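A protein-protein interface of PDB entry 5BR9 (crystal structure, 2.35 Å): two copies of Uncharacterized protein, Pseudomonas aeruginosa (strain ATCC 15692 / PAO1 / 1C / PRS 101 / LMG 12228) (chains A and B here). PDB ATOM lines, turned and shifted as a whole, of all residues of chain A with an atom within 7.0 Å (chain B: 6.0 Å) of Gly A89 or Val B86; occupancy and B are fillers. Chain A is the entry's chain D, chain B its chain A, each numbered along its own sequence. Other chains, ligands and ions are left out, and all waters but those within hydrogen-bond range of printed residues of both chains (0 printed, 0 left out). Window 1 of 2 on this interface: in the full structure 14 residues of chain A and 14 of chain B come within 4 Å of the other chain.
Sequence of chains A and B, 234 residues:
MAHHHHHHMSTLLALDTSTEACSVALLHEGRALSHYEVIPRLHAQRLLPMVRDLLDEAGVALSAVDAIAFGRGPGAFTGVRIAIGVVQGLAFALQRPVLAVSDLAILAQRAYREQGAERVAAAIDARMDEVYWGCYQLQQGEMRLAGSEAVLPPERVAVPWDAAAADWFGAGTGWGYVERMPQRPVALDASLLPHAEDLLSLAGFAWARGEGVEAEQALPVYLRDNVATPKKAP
O of Gly B85 sits close to N of Val A86.
The backbone NH (N) of Val B86 lies close to the backbone carbonyl oxygen (O) of Gly A85 (3.5 Å).
NE2 of Gln A88 sits close to O of Ala A215, 3.2 Å away.
Among the printed residues, merely in contact across the chains: Ile A82 with Arg B81 (3.6 Å), Ile A82 with Gly B85 (3.4 Å), Gly A85 with Gly B85 (3.4 Å), Val A86 with Val B86 (3.97 Å), Val A86 with Gly B89 (3.7 Å), Gln A88 with Leu B48 (3.8 Å), Gln A88 with Val B86 (3.6 Å), Gly A89 with Val B86 (3.6 Å), Gly A89 with Gly B89 (3.6 Å), Gly A89 with Leu B90 (3.4 Å), Leu A90 with Gly B89 (3.5 Å), Phe A92 with Leu B48 (3.6 Å), Phe A92 with Leu B90 (3.5 Å) and Ala A93 with Ala B93 (3.5 Å).
Gly A89 touches just these residues of chain B: Val B86, Gly B89 and Leu B90.
Val B86 touches just these residues of chain A: Gly A85 (3.3 Å), Val A86 (3.97 Å), Gln A88 (3.6 Å) and Gly A89 (3.6 Å).
Gly B85 touches three residues of chain A.
Of the printed residues of chain B, Phe A92 touches Leu B48 (3.6 Å) and Leu B90 (3.5 Å).
Of the printed residues of chain A, Ala B93 touches Ala A93 (3.5 Å).
Printed residues of chain B within 4 Å of Gly A85: Gly B85 and Val B86.
Printed residues of chain B within 4 Å of Ile A82: Arg B81 and Gly B85.
Of the printed residues of chain A, Leu B48 touches Gln A88 and Phe A92.
The nearest residue of chain B that does not touch Gly A89 is Leu B48 (4.6 Å).
Hydrophobic or aromatic side chains of chain B within 4 Å of the printed part of chain A: Leu B48, Val B86, Leu B90 and Ala B93.
Of the 16 printed residues of chain A, 8 touch a printed residue of chain B.
Printed residues of chain A that touch a printed residue of chain B: Ile A82, Gly A85, Val A86, Gln A88, Gly A89, Leu A90, Phe A92 and Ala A93.
Hydrophobic or aromatic side chains of chain A within 4 Å of the printed part of chain B: Ile A82, Val A86, Leu A90, Phe A92 and Ala A93.
Among the printed residues, no Asp or Glu carboxylate lies within 4 Å of a Lys or Arg side-chain nitrogen of the other chain.
Gly B85 touches its own counterpart, Gly A85.
Val A86 touches Gly B89, and with the chains exchanged Gly A89 touches Val B86.
Gln A88 touches Val B86, but with the chains exchanged Val A86 does not touch Gln B88 (4.3 Å).
Gly A89 touches Leu B90, and with the chains exchanged Leu A90 touches Gly B89.
Positions printed for both chains: 81, 82, 84, 85, 86, 87, 88, 89, 90, 91 and 93.
Of the 16 pairs that touch across the chains among the printed residues, 10 have their exchanged pair printed and touching as well.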
ATOM      1  N   ILE A  68     -10.333  22.841 -18.803  1.00  0.00           N
ATOM      2  CA  ILE A  68     -10.855  23.972 -18.061  1.00  0.00           C
ATOM      3  C   ILE A  68      -9.880  24.332 -16.943  1.00  0.00           C
ATOM      4  O   ILE A  68      -9.563  23.502 -16.096  1.00  0.00           O
ATOM      5  CB  ILE A  68     -12.240  23.664 -17.521  1.00  0.00           C
ATOM      6  CG1 ILE A  68     -13.150  23.196 -18.660  1.00  0.00           C
ATOM      7  CG2 ILE A  68     -12.823  24.888 -16.850  1.00  0.00           C
ATOM      8  CD1 ILE A  68     -14.510  22.781 -18.202  1.00  0.00           C
ATOM      9  N   ARG A  81     -15.588  27.838  -3.287  1.00  0.00           N
ATOM     10  CA  ARG A  81     -16.399  26.630  -3.177  1.00  0.00           C
ATOM     11  C   ARG A  81     -17.391  26.409  -4.334  1.00  0.00           C
ATOM     12  O   ARG A  81     -17.295  25.401  -5.041  1.00  0.00           O
ATOM     13  CB  ARG A  81     -17.150  26.639  -1.845  1.00  0.00           C
ATOM     14  N   ILE A  82     -18.333  27.332  -4.532  1.00  0.00           N
ATOM     15  CA  ILE A  82     -19.373  27.139  -5.545  1.00  0.00           C
ATOM     16  C   ILE A  82     -18.756  27.158  -6.942  1.00  0.00           C
ATOM     17  O   ILE A  82     -19.107  26.334  -7.780  1.00  0.00           O
ATOM     18  CB  ILE A  82     -20.515  28.192  -5.414  1.00  0.00           C
ATOM     19  CG1 ILE A  82     -21.296  27.995  -4.103  1.00  0.00           C
ATOM     20  CG2 ILE A  82     -21.466  28.117  -6.612  1.00  0.00           C
ATOM     21  CD1 ILE A  82     -22.438  29.005  -3.883  1.00  0.00           C
ATOM     22  N   ILE A  84     -15.628  26.323  -7.823  1.00  0.00           N
ATOM     23  CA  ILE A  84     -14.834  25.119  -8.057  1.00  0.00           C
ATOM     24  C   ILE A  84     -15.794  23.940  -8.334  1.00  0.00           C
ATOM     25  O   ILE A  84     -15.543  23.114  -9.218  1.00  0.00           O
ATOM     26  CB  ILE A  84     -13.858  24.874  -6.875  1.00  0.00           C
ATOM     27  CG1 ILE A  84     -12.735  25.907  -6.937  1.00  0.00           C
ATOM     28  CG2 ILE A  84     -13.261  23.487  -6.902  1.00  0.00           C
ATOM     29  CD1 ILE A  84     -11.712  25.766  -5.868  1.00  0.00           C
ATOM     30  N   GLY A  85     -16.915  23.907  -7.617  1.00  0.00           N
ATOM     31  CA  GLY A  85     -17.994  22.983  -7.920  1.00  0.00           C
ATOM     32  C   GLY A  85     -18.441  23.085  -9.366  1.00  0.00           C
ATOM     33  O   GLY A  85     -18.546  22.076 -10.062  1.00  0.00           O
ATOM     34  N   VAL A  86     -18.688  24.306  -9.829  1.00  0.00           N
ATOM     35  CA  VAL A  86     -19.054  24.531 -11.226  1.00  0.00           C
ATOM     36  C   VAL A  86     -18.000  23.910 -12.166  1.00  0.00           C
ATOM     37  O   VAL A  86     -18.348  23.208 -13.108  1.00  0.00           O
ATOM     38  CB  VAL A  86     -19.246  26.032 -11.517  1.00  0.00           C
ATOM     39  CG1 VAL A  86     -19.503  26.281 -13.010  1.00  0.00           C
ATOM     40  CG2 VAL A  86     -20.371  26.579 -10.683  1.00  0.00           C
ATOM     41  N   VAL A  87     -16.718  24.142 -11.888  1.00  0.00           N
ATOM     42  CA  VAL A  87     -15.652  23.603 -12.723  1.00  0.00           C
ATOM     43  C   VAL A  87     -15.718  22.078 -12.742  1.00  0.00           C
ATOM     44  O   VAL A  87     -15.605  21.464 -13.806  1.00  0.00           O
ATOM     45  CB  VAL A  87     -14.262  24.100 -12.246  1.00  0.00           C
ATOM     46  CG1 VAL A  87     -13.136  23.404 -13.027  1.00  0.00           C
ATOM     47  CG2 VAL A  87     -14.173  25.602 -12.400  1.00  0.00           C
ATOM     48  N   GLN A  88     -15.911  21.476 -11.570  1.00  0.00           N
ATOM     49  CA  GLN A  88     -16.082  20.028 -11.454  1.00  0.00           C
ATOM     50  C   GLN A  88     -17.219  19.509 -12.339  1.00  0.00           C
ATOM     51  O   GLN A  88     -17.019  18.616 -13.167  1.00  0.00           O
ATOM     52  CB  GLN A  88     -16.343  19.629  -9.997  1.00  0.00           C
ATOM     53  CG  GLN A  88     -15.092  19.489  -9.167  1.00  0.00           C
ATOM     54  CD  GLN A  88     -15.338  18.803  -7.829  1.00  0.00           C
ATOM     55  OE1 GLN A  88     -16.388  18.976  -7.214  1.00  0.00           O
ATOM     56  NE2 GLN A  88     -14.359  18.026  -7.373  1.00  0.00           N
ATOM     57  N   GLY A  89     -18.403  20.087 -12.164  1.00  0.00           N
ATOM     58  CA  GLY A  89     -19.583  19.722 -12.938  1.00  0.00           C
ATOM     59  C   GLY A  89     -19.386  19.834 -14.438  1.00  0.00           C
ATOM     60  O   GLY A  89     -19.692  18.896 -15.180  1.00  0.00           O
ATOM     61  N   LEU A  90     -18.876  20.978 -14.889  1.00  0.00           N
ATOM     62  CA  LEU A  90     -18.603  21.170 -16.308  1.00  0.00           C
ATOM     63  C   LEU A  90     -17.641  20.087 -16.844  1.00  0.00           C
ATOM     64  O   LEU A  90     -17.929  19.418 -17.830  1.00  0.00           O
ATOM     65  CB  LEU A  90     -18.001  22.554 -16.557  1.00  0.00           C
ATOM     66  CG  LEU A  90     -18.777  23.850 -16.321  1.00  0.00           C
ATOM     67  CD1 LEU A  90     -17.810  25.024 -16.470  1.00  0.00           C
ATOM     68  CD2 LEU A  90     -19.909  23.965 -17.319  1.00  0.00           C
ATOM     69  N   ALA A  91     -16.508  19.919 -16.167  1.00  0.00           N
ATOM     70  CA  ALA A  91     -15.459  19.011 -16.610  1.00  0.00           C
ATOM     71  C   ALA A  91     -15.939  17.571 -16.638  1.00  0.00           C
ATOM     72  O   ALA A  91     -15.591  16.822 -17.538  1.00  0.00           O
ATOM     73  CB  ALA A  91     -14.254  19.132 -15.719  1.00  0.00           C
ATOM     74  N   PHE A  92     -16.741  17.195 -15.647  1.00  0.00           N
ATOM     75  CA  PHE A  92     -17.293  15.852 -15.578  1.00  0.00           C
ATOM     76  C   PHE A  92     -18.263  15.580 -16.744  1.00  0.00           C
ATOM     77  O   PHE A  92     -18.161  14.564 -17.434  1.00  0.00           O
ATOM     78  CB  PHE A  92     -17.989  15.668 -14.235  1.00  0.00           C
ATOM     79  CG  PHE A  92     -18.614  14.319 -14.039  1.00  0.00           C
ATOM     80  CD1 PHE A  92     -17.879  13.273 -13.485  1.00  0.00           C
ATOM     81  CD2 PHE A  92     -19.950  14.096 -14.393  1.00  0.00           C
ATOM     82  CE1 PHE A  92     -18.466  12.027 -13.272  1.00  0.00           C
ATOM     83  CE2 PHE A  92     -20.547  12.853 -14.181  1.00  0.00           C
ATOM     84  CZ  PHE A  92     -19.797  11.816 -13.620  1.00  0.00           C
ATOM     85  N   ALA A  93     -19.195  16.504 -16.954  1.00  0.00           N
ATOM     86  CA  ALA A  93     -20.190  16.375 -18.010  1.00  0.00           C
ATOM     87  C   ALA A  93     -19.550  16.381 -19.391  1.00  0.00           C
ATOM     88  O   ALA A  93     -20.010  15.692 -20.297  1.00  0.00           O
ATOM     89  CB  ALA A  93     -21.235  17.497 -17.894  1.00  0.00           C
ATOM     90  N   LEU A  94     -18.477  17.147 -19.542  1.00  0.00           N
ATOM     91  CA  LEU A  94     -17.790  17.263 -20.819  1.00  0.00           C
ATOM     92  C   LEU A  94     -16.760  16.165 -21.034  1.00  0.00           C
ATOM     93  O   LEU A  94     -16.276  15.980 -22.168  1.00  0.00           O
ATOM     94  CB  LEU A  94     -17.096  18.619 -20.933  1.00  0.00           C
ATOM     95  CG  LEU A  94     -18.003  19.856 -20.971  1.00  0.00           C
ATOM     96  CD1 LEU A  94     -17.146  21.141 -20.930  1.00  0.00           C
ATOM     97  CD2 LEU A  94     -18.954  19.819 -22.191  1.00  0.00           C
ATOM     98  N   GLN A  95     -16.432  15.453 -19.957  1.00  0.00           N
ATOM     99  CA  GLN A  95     -15.325  14.481 -19.930  1.00  0.00           C
ATOM    100  C   GLN A  95     -14.001  15.141 -20.326  1.00  0.00           C
ATOM    101  O   GLN A  95     -13.362  14.731 -21.281  1.00  0.00           O
ATOM    102  CB  GLN A  95     -15.604  13.297 -20.867  1.00  0.00           C
ATOM    103  CG  GLN A  95     -16.780  12.410 -20.504  1.00  0.00           C
ATOM    104  CD  GLN A  95     -16.784  11.107 -21.312  1.00  0.00           C
ATOM    105  OE1 GLN A  95     -16.730  11.119 -22.544  1.00  0.00           O
ATOM    106  NE2 GLN A  95     -16.824   9.983 -20.612  1.00  0.00           N
ATOM    107  N   ALA A 215     -11.825  15.689 -13.107  1.00  0.00           N
ATOM    108  CA  ALA A 215     -12.753  16.596 -12.431  1.00  0.00           C
ATOM    109  C   ALA A 215     -12.863  16.378 -10.919  1.00  0.00           C
ATOM    110  O   ALA A 215     -12.961  17.339 -10.159  1.00  0.00           O
ATOM    111  CB  ALA A 215     -14.140  16.482 -13.071  1.00  0.00           C
ATOM    112  N   LEU B  15     -28.963  14.249  -6.138  1.00  0.00           N
ATOM    113  CA  LEU B  15     -27.817  14.165  -5.244  1.00  0.00           C
ATOM    114  C   LEU B  15     -27.980  15.031  -3.988  1.00  0.00           C
ATOM    115  O   LEU B  15     -28.588  16.106  -4.026  1.00  0.00           O
ATOM    116  CB  LEU B  15     -26.534  14.489  -5.984  1.00  0.00           C
ATOM    117  CG  LEU B  15     -26.290  15.834  -6.608  1.00  0.00           C
ATOM    118  CD1 LEU B  15     -25.749  16.777  -5.534  1.00  0.00           C
ATOM    119  CD2 LEU B  15     -25.281  15.611  -7.742  1.00  0.00           C
ATOM    120  N   LEU B  47     -18.302  12.820  -4.554  1.00  0.00           N
ATOM    121  CA  LEU B  47     -19.606  13.009  -5.178  1.00  0.00           C
ATOM    122  C   LEU B  47     -19.650  12.541  -6.636  1.00  0.00           C
ATOM    123  O   LEU B  47     -20.506  11.738  -7.011  1.00  0.00           O
ATOM    124  CB  LEU B  47     -20.033  14.476  -5.107  1.00  0.00           C
ATOM    125  CG  LEU B  47     -21.391  14.756  -5.755  1.00  0.00           C
ATOM    126  CD1 LEU B  47     -22.444  13.923  -5.064  1.00  0.00           C
ATOM    127  CD2 LEU B  47     -21.745  16.237  -5.644  1.00  0.00           C
ATOM    128  N   LEU B  48     -18.746  13.054  -7.464  1.00  0.00           N
ATOM    129  CA  LEU B  48     -18.755  12.695  -8.881  1.00  0.00           C
ATOM    130  C   LEU B  48     -18.430  11.216  -9.140  1.00  0.00           C
ATOM    131  O   LEU B  48     -18.988  10.625 -10.052  1.00  0.00           O
ATOM    132  CB  LEU B  48     -17.806  13.594  -9.664  1.00  0.00           C
ATOM    133  CG  LEU B  48     -18.348  15.029  -9.746  1.00  0.00           C
ATOM    134  CD1 LEU B  48     -17.404  15.914 -10.564  1.00  0.00           C
ATOM    135  CD2 LEU B  48     -19.785  15.084 -10.283  1.00  0.00           C
ATOM    136  N   ARG B  81     -22.994  24.142  -0.689  1.00  0.00           N
ATOM    137  CA  ARG B  81     -22.329  24.938  -1.720  1.00  0.00           C
ATOM    138  C   ARG B  81     -21.679  24.074  -2.788  1.00  0.00           C
ATOM    139  O   ARG B  81     -21.701  24.419  -3.964  1.00  0.00           O
ATOM    140  CB  ARG B  81     -21.297  25.870  -1.088  1.00  0.00           C
ATOM    141  CG  ARG B  81     -21.949  27.098  -0.489  1.00  0.00           C
ATOM    142  CD  ARG B  81     -21.132  27.771   0.591  1.00  0.00           C
ATOM    143  NE  ARG B  81     -22.031  28.482   1.501  1.00  0.00           N
ATOM    144  CZ  ARG B  81     -22.549  29.685   1.261  1.00  0.00           C
ATOM    145  NH1 ARG B  81     -23.367  30.240   2.146  1.00  0.00           N
ATOM    146  NH2 ARG B  81     -22.247  30.334   0.138  1.00  0.00           N
ATOM    147  N   ILE B  82     -21.114  22.946  -2.376  1.00  0.00           N
ATOM    148  CA  ILE B  82     -20.581  21.978  -3.322  1.00  0.00           C
ATOM    149  C   ILE B  82     -21.685  21.448  -4.241  1.00  0.00           C
ATOM    150  O   ILE B  82     -21.526  21.427  -5.465  1.00  0.00           O
ATOM    151  CB  ILE B  82     -19.879  20.829  -2.582  1.00  0.00           C
ATOM    152  CG1 ILE B  82     -18.597  21.329  -1.916  1.00  0.00           C
ATOM    153  CG2 ILE B  82     -19.568  19.678  -3.526  1.00  0.00           C
ATOM    154  CD1 ILE B  82     -18.153  20.450  -0.741  1.00  0.00           C
ATOM    155  N   ALA B  83     -22.798  21.013  -3.657  1.00  0.00           N
ATOM    156  CA  ALA B  83     -23.913  20.526  -4.465  1.00  0.00           C
ATOM    157  C   ALA B  83     -24.349  21.591  -5.461  1.00  0.00           C
ATOM    158  O   ALA B  83     -24.512  21.299  -6.645  1.00  0.00           O
ATOM    159  CB  ALA B  83     -25.101  20.100  -3.579  1.00  0.00           C
ATOM    160  N   ILE B  84     -24.506  22.830  -4.987  1.00  0.00           N
ATOM    161  CA  ILE B  84     -24.972  23.910  -5.849  1.00  0.00           C
ATOM    162  C   ILE B  84     -24.082  24.070  -7.095  1.00  0.00           C
ATOM    163  O   ILE B  84     -24.578  24.033  -8.234  1.00  0.00           O
ATOM    164  CB  ILE B  84     -25.072  25.221  -5.070  1.00  0.00           C
ATOM    165  CG1 ILE B  84     -26.233  25.147  -4.085  1.00  0.00           C
ATOM    166  CG2 ILE B  84     -25.254  26.393  -6.022  1.00  0.00           C
ATOM    167  CD1 ILE B  84     -26.312  26.311  -3.114  1.00  0.00           C
ATOM    168  N   GLY B  85     -22.776  24.224  -6.885  1.00  0.00           N
ATOM    169  CA  GLY B  85     -21.841  24.390  -7.986  1.00  0.00           C
ATOM    170  C   GLY B  85     -21.781  23.237  -8.974  1.00  0.00           C
ATOM    171  O   GLY B  85     -21.884  23.422 -10.197  1.00  0.00           O
ATOM    172  N   VAL B  86     -21.631  22.033  -8.448  1.00  0.00           N
ATOM    173  CA  VAL B  86     -21.509  20.865  -9.298  1.00  0.00           C
ATOM    174  C   VAL B  86     -22.773  20.667 -10.144  1.00  0.00           C
ATOM    175  O   VAL B  86     -22.690  20.435 -11.352  1.00  0.00           O
ATOM    176  CB  VAL B  86     -21.188  19.615  -8.450  1.00  0.00           C
ATOM    177  CG1 VAL B  86     -21.281  18.344  -9.291  1.00  0.00           C
ATOM    178  CG2 VAL B  86     -19.800  19.760  -7.817  1.00  0.00           C
ATOM    179  N   VAL B  87     -23.938  20.787  -9.519  1.00  0.00           N
ATOM    180  CA  VAL B  87     -25.193  20.604 -10.233  1.00  0.00           C
ATOM    181  C   VAL B  87     -25.328  21.663 -11.342  1.00  0.00           C
ATOM    182  O   VAL B  87     -25.672  21.349 -12.480  1.00  0.00           O
ATOM    183  CB  VAL B  87     -26.385  20.633  -9.254  1.00  0.00           C
ATOM    184  CG1 VAL B  87     -27.677  20.749  -9.998  1.00  0.00           C
ATOM    185  CG2 VAL B  87     -26.382  19.371  -8.410  1.00  0.00           C
ATOM    186  N   GLN B  88     -25.011  22.910 -11.017  1.00  0.00           N
ATOM    187  CA  GLN B  88     -25.023  23.992 -11.995  1.00  0.00           C
ATOM    188  C   GLN B  88     -24.076  23.726 -13.174  1.00  0.00           C
ATOM    189  O   GLN B  88     -24.408  24.000 -14.325  1.00  0.00           O
ATOM    190  CB  GLN B  88     -24.654  25.306 -11.308  1.00  0.00           C
ATOM    191  CG  GLN B  88     -25.837  25.962 -10.577  1.00  0.00           C
ATOM    192  CD  GLN B  88     -25.485  27.340 -10.007  1.00  0.00           C
ATOM    193  OE1 GLN B  88     -26.242  28.291 -10.155  1.00  0.00           O
ATOM    194  NE2 GLN B  88     -24.328  27.438  -9.348  1.00  0.00           N
ATOM    195  N   GLY B  89     -22.870  23.251 -12.876  1.00  0.00           N
ATOM    196  CA  GLY B  89     -21.909  22.912 -13.913  1.00  0.00           C
ATOM    197  C   GLY B  89     -22.394  21.772 -14.807  1.00  0.00           C
ATOM    198  O   GLY B  89     -22.319  21.854 -16.036  1.00  0.00           O
ATOM    199  N   LEU B  90     -22.905  20.716 -14.180  1.00  0.00           N
ATOM    200  CA  LEU B  90     -23.427  19.555 -14.884  1.00  0.00           C
ATOM    201  C   LEU B  90     -24.532  20.025 -15.812  1.00  0.00           C
ATOM    202  O   LEU B  90     -24.542  19.700 -17.000  1.00  0.00           O
ATOM    203  CB  LEU B  90     -23.964  18.500 -13.907  1.00  0.00           C
ATOM    204  CG  LEU B  90     -23.003  17.699 -13.037  1.00  0.00           C
ATOM    205  CD1 LEU B  90     -23.804  16.808 -12.127  1.00  0.00           C
ATOM    206  CD2 LEU B  90     -22.060  16.846 -13.892  1.00  0.00           C
ATOM    207  N   ALA B  91     -25.439  20.820 -15.249  1.00  0.00           N
ATOM    208  CA  ALA B  91     -26.650  21.220 -15.932  1.00  0.00           C
ATOM    209  C   ALA B  91     -26.371  22.181 -17.069  1.00  0.00           C
ATOM    210  O   ALA B  91     -27.009  22.104 -18.110  1.00  0.00           O
ATOM    211  CB  ALA B  91     -27.626  21.836 -14.945  1.00  0.00           C
ATOM    212  N   ALA B  93     -23.588  22.268 -18.854  1.00  0.00           N
ATOM    213  CA  ALA B  93     -22.938  21.508 -19.909  1.00  0.00           C
ATOM    214  C   ALA B  93     -23.922  20.627 -20.677  1.00  0.00           C
ATOM    215  O   ALA B  93     -23.812  20.512 -21.893  1.00  0.00           O
ATOM    216  CB  ALA B  93     -21.825  20.674 -19.332  1.00  0.00           C
